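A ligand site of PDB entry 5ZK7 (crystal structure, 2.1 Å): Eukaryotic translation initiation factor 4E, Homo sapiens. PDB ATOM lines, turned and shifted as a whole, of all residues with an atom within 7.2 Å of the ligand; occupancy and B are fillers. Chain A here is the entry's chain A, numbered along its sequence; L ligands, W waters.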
ATOM      1  N   PHE A  22       7.265  -0.488 -22.537  1.00  0.00           N
ATOM      2  CA  PHE A  22       8.713  -0.353 -22.484  1.00  0.00           C
ATOM      3  C   PHE A  22       9.053   1.122 -22.310  1.00  0.00           C
ATOM      4  O   PHE A  22       8.404   1.968 -22.932  1.00  0.00           O
ATOM      5  CB  PHE A  22       9.328  -0.878 -23.781  1.00  0.00           C
ATOM      6  CG  PHE A  22      10.838  -0.922 -23.773  1.00  0.00           C
ATOM      7  CD1 PHE A  22      11.581   0.198 -24.131  1.00  0.00           C
ATOM      8  CD2 PHE A  22      11.505  -2.088 -23.424  1.00  0.00           C
ATOM      9  CE1 PHE A  22      12.969   0.155 -24.130  1.00  0.00           C
ATOM     10  CE2 PHE A  22      12.893  -2.131 -23.423  1.00  0.00           C
ATOM     11  CZ  PHE A  22      13.626  -1.010 -23.783  1.00  0.00           C
ATOM     12  N   TRP A  30      17.849  -3.938 -20.769  1.00  0.00           N
ATOM     13  CA  TRP A  30      16.731  -3.857 -21.720  1.00  0.00           C
ATOM     14  C   TRP A  30      15.494  -4.561 -21.173  1.00  0.00           C
ATOM     15  O   TRP A  30      14.417  -3.969 -21.098  1.00  0.00           O
ATOM     16  CB  TRP A  30      17.145  -4.449 -23.073  1.00  0.00           C
ATOM     17  CG  TRP A  30      16.197  -4.120 -24.186  1.00  0.00           C
ATOM     18  CD1 TRP A  30      16.270  -3.040 -25.021  1.00  0.00           C
ATOM     19  CD2 TRP A  30      15.037  -4.861 -24.584  1.00  0.00           C
ATOM     20  NE1 TRP A  30      15.223  -3.069 -25.923  1.00  0.00           N
ATOM     21  CE2 TRP A  30      14.450  -4.175 -25.666  1.00  0.00           C
ATOM     22  CE3 TRP A  30      14.441  -6.045 -24.118  1.00  0.00           C
ATOM     23  CZ2 TRP A  30      13.286  -4.627 -26.306  1.00  0.00           C
ATOM     24  CZ3 TRP A  30      13.277  -6.497 -24.759  1.00  0.00           C
ATOM     25  CH2 TRP A  30      12.722  -5.786 -25.838  1.00  0.00           C
ATOM     26  N   GLN A  31      15.654  -5.832 -20.799  1.00  0.00           N
ATOM     27  CA  GLN A  31      14.564  -6.623 -20.214  1.00  0.00           C
ATOM     28  C   GLN A  31      14.131  -6.139 -18.820  1.00  0.00           C
ATOM     29  O   GLN A  31      13.080  -6.551 -18.330  1.00  0.00           O
ATOM     30  CB  GLN A  31      14.947  -8.107 -20.156  1.00  0.00           C
ATOM     31  N   GLY A  62      11.333   6.968 -27.131  1.00  0.00           N
ATOM     32  CA  GLY A  62      11.956   5.707 -26.712  1.00  0.00           C
ATOM     33  C   GLY A  62      11.057   4.733 -25.945  1.00  0.00           C
ATOM     34  O   GLY A  62      11.548   3.721 -25.445  1.00  0.00           O
ATOM     35  N   ASP A  64       7.679   2.043 -25.862  1.00  0.00           N
ATOM     36  CA  ASP A  64       6.845   1.169 -26.691  1.00  0.00           C
ATOM     37  C   ASP A  64       5.589   0.740 -25.945  1.00  0.00           C
ATOM     38  O   ASP A  64       5.596   0.609 -24.731  1.00  0.00           O
ATOM     39  CB  ASP A  64       7.558  -0.143 -27.082  1.00  0.00           C
ATOM     40  CG  ASP A  64       8.973   0.043 -27.571  1.00  0.00           C
ATOM     41  OD1 ASP A  64       9.251   1.000 -28.317  1.00  0.00           O
ATOM     42  OD2 ASP A  64       9.799  -0.815 -27.235  1.00  0.00           O
ATOM     43  N   PRO A  74       7.071 -10.059 -25.420  1.00  0.00           N
ATOM     44  CA  PRO A  74       7.347  -9.236 -26.598  1.00  0.00           C
ATOM     45  C   PRO A  74       8.847  -9.025 -26.821  1.00  0.00           C
ATOM     46  O   PRO A  74       9.357  -7.895 -26.715  1.00  0.00           O
ATOM     47  CB  PRO A  74       6.631  -7.921 -26.244  1.00  0.00           C
ATOM     48  CG  PRO A  74       6.831  -7.805 -24.781  1.00  0.00           C
ATOM     49  CD  PRO A  74       6.672  -9.220 -24.271  1.00  0.00           C
ATOM     50  N   MET A  75       9.552 -10.106 -27.150  1.00  0.00           N
ATOM     51  CA  MET A  75      10.990 -10.080 -27.367  1.00  0.00           C
ATOM     52  C   MET A  75      11.392 -11.199 -28.319  1.00  0.00           C
ATOM     53  O   MET A  75      10.735 -12.253 -28.367  1.00  0.00           O
ATOM     54  CB  MET A  75      11.742 -10.199 -26.028  1.00  0.00           C
ATOM     55  CG  MET A  75      11.649 -11.569 -25.360  1.00  0.00           C
ATOM     56  SD  MET A  75      11.890 -11.530 -23.568  1.00  0.00           S
ATOM     57  CE  MET A  75      13.296 -10.421 -23.386  1.00  0.00           C
ATOM     58  N   TRP A  76      12.465 -10.970 -29.077  1.00  0.00           N
ATOM     59  CA  TRP A  76      12.924 -11.914 -30.122  1.00  0.00           C
ATOM     60  C   TRP A  76      13.168 -13.318 -29.570  1.00  0.00           C
ATOM     61  O   TRP A  76      12.854 -14.306 -30.239  1.00  0.00           O
ATOM     62  CB  TRP A  76      14.237 -11.445 -30.768  1.00  0.00           C
ATOM     63  CG  TRP A  76      14.222 -10.067 -31.355  1.00  0.00           C
ATOM     64  CD1 TRP A  76      13.201  -9.474 -32.046  1.00  0.00           C
ATOM     65  CD2 TRP A  76      15.282  -9.110 -31.323  1.00  0.00           C
ATOM     66  NE1 TRP A  76      13.565  -8.209 -32.433  1.00  0.00           N
ATOM     67  CE2 TRP A  76      14.840  -7.959 -31.999  1.00  0.00           C
ATOM     68  CE3 TRP A  76      16.577  -9.115 -30.771  1.00  0.00           C
ATOM     69  CZ2 TRP A  76      15.638  -6.809 -32.149  1.00  0.00           C
ATOM     70  CZ3 TRP A  76      17.373  -7.979 -30.919  1.00  0.00           C
ATOM     71  CH2 TRP A  76      16.901  -6.847 -31.606  1.00  0.00           C
ATOM     72  N   GLU A  77      13.702 -13.394 -28.348  1.00  0.00           N
ATOM     73  CA  GLU A  77      14.170 -14.652 -27.761  1.00  0.00           C
ATOM     74  C   GLU A  77      13.078 -15.617 -27.262  1.00  0.00           C
ATOM     75  O   GLU A  77      13.385 -16.770 -26.950  1.00  0.00           O
ATOM     76  CB  GLU A  77      15.177 -14.367 -26.619  1.00  0.00           C
ATOM     77  CG  GLU A  77      16.564 -13.924 -27.082  1.00  0.00           C
ATOM     78  CD  GLU A  77      16.663 -12.457 -27.516  1.00  0.00           C
ATOM     79  OE1 GLU A  77      17.528 -12.156 -28.380  1.00  0.00           O
ATOM     80  OE2 GLU A  77      15.907 -11.607 -27.005  1.00  0.00           O
ATOM     81  N   ASP A  78      11.822 -15.159 -27.186  1.00  0.00           N
ATOM     82  CA  ASP A  78      10.702 -16.042 -26.811  1.00  0.00           C
ATOM     83  C   ASP A  78      10.558 -17.165 -27.853  1.00  0.00           C
ATOM     84  O   ASP A  78      10.782 -16.940 -29.046  1.00  0.00           O
ATOM     85  CB  ASP A  78       9.394 -15.244 -26.704  1.00  0.00           C
ATOM     86  CG  ASP A  78       8.234 -16.072 -26.141  1.00  0.00           C
ATOM     87  OD1 ASP A  78       7.685 -16.934 -26.855  1.00  0.00           O
ATOM     88  OD2 ASP A  78       7.850 -15.827 -24.975  1.00  0.00           O
ATOM     89  N   ASN A  81       8.585 -16.404 -30.838  1.00  0.00           N
ATOM     90  CA  ASN A  81       9.176 -15.338 -31.658  1.00  0.00           C
ATOM     91  C   ASN A  81      10.511 -15.687 -32.343  1.00  0.00           C
ATOM     92  O   ASN A  81      10.758 -15.190 -33.445  1.00  0.00           O
ATOM     93  CB  ASN A  81       9.362 -14.069 -30.803  1.00  0.00           C
ATOM     94  CG  ASN A  81       8.038 -13.467 -30.346  1.00  0.00           C
ATOM     95  OD1 ASN A  81       6.999 -13.628 -30.996  1.00  0.00           O
ATOM     96  ND2 ASN A  81       8.064 -12.744 -29.236  1.00  0.00           N
ATOM     97  N   ARG A  86       8.527  -9.759 -38.534  1.00  0.00           N
ATOM     98  CA  ARG A  86       7.548  -8.698 -38.388  1.00  0.00           C
ATOM     99  C   ARG A  86       7.255  -7.982 -39.704  1.00  0.00           C
ATOM    100  O   ARG A  86       8.159  -7.772 -40.498  1.00  0.00           O
ATOM    101  CB  ARG A  86       8.006  -7.686 -37.334  1.00  0.00           C
ATOM    102  CG  ARG A  86       9.167  -6.800 -37.760  1.00  0.00           C
ATOM    103  CD  ARG A  86       9.689  -5.917 -36.633  1.00  0.00           C
ATOM    104  NE  ARG A  86      10.783  -5.063 -37.102  1.00  0.00           N
ATOM    105  CZ  ARG A  86      11.365  -4.091 -36.397  1.00  0.00           C
ATOM    106  NH1 ARG A  86      12.357  -3.392 -36.951  1.00  0.00           N
ATOM    107  NH2 ARG A  86      10.984  -3.789 -35.158  1.00  0.00           N
ATOM    108  N   VAL A 127       3.764  -4.356 -31.883  1.00  0.00           N
ATOM    109  CA  VAL A 127       4.585  -3.405 -31.154  1.00  0.00           C
ATOM    110  C   VAL A 127       4.518  -2.063 -31.861  1.00  0.00           C
ATOM    111  O   VAL A 127       4.597  -2.009 -33.086  1.00  0.00           O
ATOM    112  CB  VAL A 127       6.074  -3.850 -31.102  1.00  0.00           C
ATOM    113  CG1 VAL A 127       6.902  -2.886 -30.243  1.00  0.00           C
ATOM    114  CG2 VAL A 127       6.199  -5.264 -30.578  1.00  0.00           C
ATOM    115  N   ASN A 129       6.642   1.535 -31.682  1.00  0.00           N
ATOM    116  CA  ASN A 129       7.809   2.244 -31.178  1.00  0.00           C
ATOM    117  C   ASN A 129       7.584   3.738 -31.354  1.00  0.00           C
ATOM    118  O   ASN A 129       7.370   4.207 -32.477  1.00  0.00           O
ATOM    119  CB  ASN A 129       9.063   1.837 -31.956  1.00  0.00           C
ATOM    120  CG  ASN A 129       9.266   0.337 -31.986  1.00  0.00           C
ATOM    121  OD1 ASN A 129       9.278  -0.266 -33.069  1.00  0.00           O
ATOM    122  ND2 ASN A 129       9.416  -0.277 -30.825  1.00  0.00           N
ATOM    123  N   ARG A 131       9.363   7.115 -31.367  1.00  0.00           N
ATOM    124  CA  ARG A 131      10.750   7.575 -31.557  1.00  0.00           C
ATOM    125  C   ARG A 131      10.815   8.968 -32.175  1.00  0.00           C
ATOM    126  O   ARG A 131       9.903   9.378 -32.901  1.00  0.00           O
ATOM    127  CB  ARG A 131      11.508   6.593 -32.470  1.00  0.00           C
ATOM    128  CG  ARG A 131      11.588   5.159 -31.987  1.00  0.00           C
ATOM    129  CD  ARG A 131      12.483   5.022 -30.765  1.00  0.00           C
ATOM    130  NE  ARG A 131      12.600   3.618 -30.352  1.00  0.00           N
ATOM    131  CZ  ARG A 131      11.760   2.978 -29.539  1.00  0.00           C
ATOM    132  NH1 ARG A 131      10.696   3.570 -29.005  1.00  0.00           N
ATOM    133  NH2 ARG A 131      11.997   1.695 -29.259  1.00  0.00           N
ATOM    134  N   LYS A 136       7.289   3.721 -35.448  1.00  0.00           N
ATOM    135  CA  LYS A 136       7.178   2.419 -36.126  1.00  0.00           C
ATOM    136  C   LYS A 136       6.097   1.556 -35.464  1.00  0.00           C
ATOM    137  O   LYS A 136       5.972   1.544 -34.246  1.00  0.00           O
ATOM    138  CB  LYS A 136       8.513   1.678 -36.077  1.00  0.00           C
ATOM    139  CG  LYS A 136       9.599   2.317 -36.939  1.00  0.00           C
ATOM    140  CD  LYS A 136      10.937   1.609 -36.785  1.00  0.00           C
ATOM    141  CE  LYS A 136      11.541   1.815 -35.400  1.00  0.00           C
ATOM    142  NZ  LYS A 136      13.005   1.549 -35.385  1.00  0.00           N
ATOM    143  N   TRP A 140       4.060  -8.900 -35.298  1.00  0.00           N
ATOM    144  CA  TRP A 140       5.016  -9.980 -35.126  1.00  0.00           C
ATOM    145  C   TRP A 140       4.323 -11.331 -35.365  1.00  0.00           C
ATOM    146  O   TRP A 140       3.301 -11.609 -34.735  1.00  0.00           O
ATOM    147  CB  TRP A 140       5.582  -9.959 -33.701  1.00  0.00           C
ATOM    148  CG  TRP A 140       6.608  -8.885 -33.430  1.00  0.00           C
ATOM    149  CD1 TRP A 140       6.667  -7.627 -33.987  1.00  0.00           C
ATOM    150  CD2 TRP A 140       7.692  -8.958 -32.508  1.00  0.00           C
ATOM    151  NE1 TRP A 140       7.727  -6.932 -33.471  1.00  0.00           N
ATOM    152  CE2 TRP A 140       8.375  -7.723 -32.545  1.00  0.00           C
ATOM    153  CE3 TRP A 140       8.154  -9.953 -31.639  1.00  0.00           C
ATOM    154  CZ2 TRP A 140       9.502  -7.466 -31.769  1.00  0.00           C
ATOM    155  CZ3 TRP A 140       9.269  -9.702 -30.857  1.00  0.00           C
ATOM    156  CH2 TRP A 140       9.939  -8.454 -30.927  1.00  0.00           C
ATOM    157  N   HIS A 174      13.315 -11.714 -37.528  1.00  0.00           N
ATOM    158  CA  HIS A 174      13.979 -11.241 -36.306  1.00  0.00           C
ATOM    159  C   HIS A 174      15.472 -11.618 -36.292  1.00  0.00           C
ATOM    160  O   HIS A 174      16.280 -10.916 -35.684  1.00  0.00           O
ATOM    161  CB  HIS A 174      13.288 -11.778 -35.046  1.00  0.00           C
ATOM    162  CG  HIS A 174      11.903 -11.247 -34.844  1.00  0.00           C
ATOM    163  ND1 HIS A 174      11.574  -9.916 -34.995  1.00  0.00           N
ATOM    164  CD2 HIS A 174      10.760 -11.875 -34.471  1.00  0.00           C
ATOM    165  CE1 HIS A 174      10.292  -9.750 -34.740  1.00  0.00           C
ATOM    166  NE2 HIS A 174       9.768 -10.917 -34.423  1.00  0.00           N
ATOM    167  N   THR A 177      17.357  -8.938 -38.243  1.00  0.00           N
ATOM    168  CA  THR A 177      17.360  -7.696 -37.460  1.00  0.00           C
ATOM    169  C   THR A 177      18.356  -7.759 -36.295  1.00  0.00           C
ATOM    170  O   THR A 177      18.875  -6.722 -35.856  1.00  0.00           O
ATOM    171  CB  THR A 177      15.939  -7.366 -36.919  1.00  0.00           C
ATOM    172  OG1 THR A 177      14.980  -7.440 -37.986  1.00  0.00           O
ATOM    173  CG2 THR A 177      15.888  -5.971 -36.304  1.00  0.00           C
HETATM  174  O1  LIG L   1      14.612   0.337 -32.035  1.00  0.00           O
HETATM  175  P1  LIG L   1      14.191  -1.012 -31.247  1.00  0.00           P
HETATM  176  O2  LIG L   1      13.420  -0.632 -30.016  1.00  0.00           O
HETATM  177  O3  LIG L   1      13.596  -1.980 -32.252  1.00  0.00           O
HETATM  178  O4  LIG L   1      15.617  -1.605 -30.796  1.00  0.00           O
HETATM  179  C1  LIG L   1      16.622  -0.800 -30.195  1.00  0.00           C
HETATM  180  C2  LIG L   1      17.569  -1.671 -29.379  1.00  0.00           C
HETATM  181  O5  LIG L   1      16.864  -2.407 -28.370  1.00  0.00           O
HETATM  182  C3  LIG L   1      18.317  -2.708 -30.221  1.00  0.00           C
HETATM  183  O6  LIG L   1      19.592  -2.203 -30.655  1.00  0.00           O
HETATM  184  C4  LIG L   1      18.442  -3.921 -29.318  1.00  0.00           C
HETATM  185  O7  LIG L   1      19.736  -3.997 -28.692  1.00  0.00           O
HETATM  186  C5  LIG L   1      17.354  -3.749 -28.261  1.00  0.00           C
HETATM  187  N1  LIG L   1      16.295  -4.788 -28.448  1.00  0.00           N
HETATM  188  C6  LIG L   1      15.187  -4.384 -29.324  1.00  0.00           C
HETATM  189  N2  LIG L   1      14.435  -5.627 -29.248  1.00  0.00           N
HETATM  190  C7  LIG L   1      13.180  -5.582 -30.045  1.00  0.00           C
HETATM  191  C8  LIG L   1      14.987  -6.576 -28.500  1.00  0.00           C
HETATM  192  C9  LIG L   1      14.595  -7.956 -28.145  1.00  0.00           C
HETATM  193  O8  LIG L   1      13.547  -8.479 -28.574  1.00  0.00           O
HETATM  194  N3  LIG L   1      15.430  -8.648 -27.337  1.00  0.00           N
HETATM  195  C10 LIG L   1      16.582  -8.112 -26.855  1.00  0.00           C
HETATM  196  N4  LIG L   1      17.358  -8.860 -26.042  1.00  0.00           N
HETATM  197  N5  LIG L   1      17.000  -6.835 -27.140  1.00  0.00           N
HETATM  198  C11 LIG L   1      16.250  -6.033 -27.955  1.00  0.00           C
HETATM  199  O   HOH W   1      12.321  -1.658 -27.821  1.00  0.00           O
HETATM  200  O   HOH W   2      10.582  -3.631 -31.251  1.00  0.00           O
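The side-chain amino group (NZ) of Lys 136 lies within salt-bridge range of an oxygen (O1) of the ligand (3.9 Å).
The indole nitrogen (NE1) of Trp 30 sits at hydrogen-bond distance from an oxygen (O5) of the ligand.
An oxygen (O8) of the ligand is in hydrogen-bond range of the backbone NH (N) of Trp 76.
NH2 of Arg 131 is in salt-bridge range of O2 of the ligand.
The side-chain carboxylate (OE2) of Glu 77 lies within hydrogen-bond range of a nitrogen (N3) of the ligand (3.0 Å).
The backbone carbonyl oxygen of Lys 136 sits at hydrogen-bond distance from the backbone NH of Asn 129, 2.7 Å away.
NH2 of Arg 131 lies within salt-bridge range of OD1 of Asp 64 (3.0 Å).
The backbone carbonyl oxygen of Met 75 sits at hydrogen-bond distance from the side-chain amide nitrogen of Asn 81.
CA of Met 75 touches O8 of the ligand, at 3.2 Å.
Six residues have an atom within 4 Å of the ligand: Trp 30, Met 75, Trp 76, Glu 77, Arg 131 and Lys 136.
The nearest printed residue that does not touch the ligand is Asn 129 (4.1 Å).
Water W1 bridges O2 of the ligand (2.7 Å) and OD2 of Asp 64 (2.7 Å).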
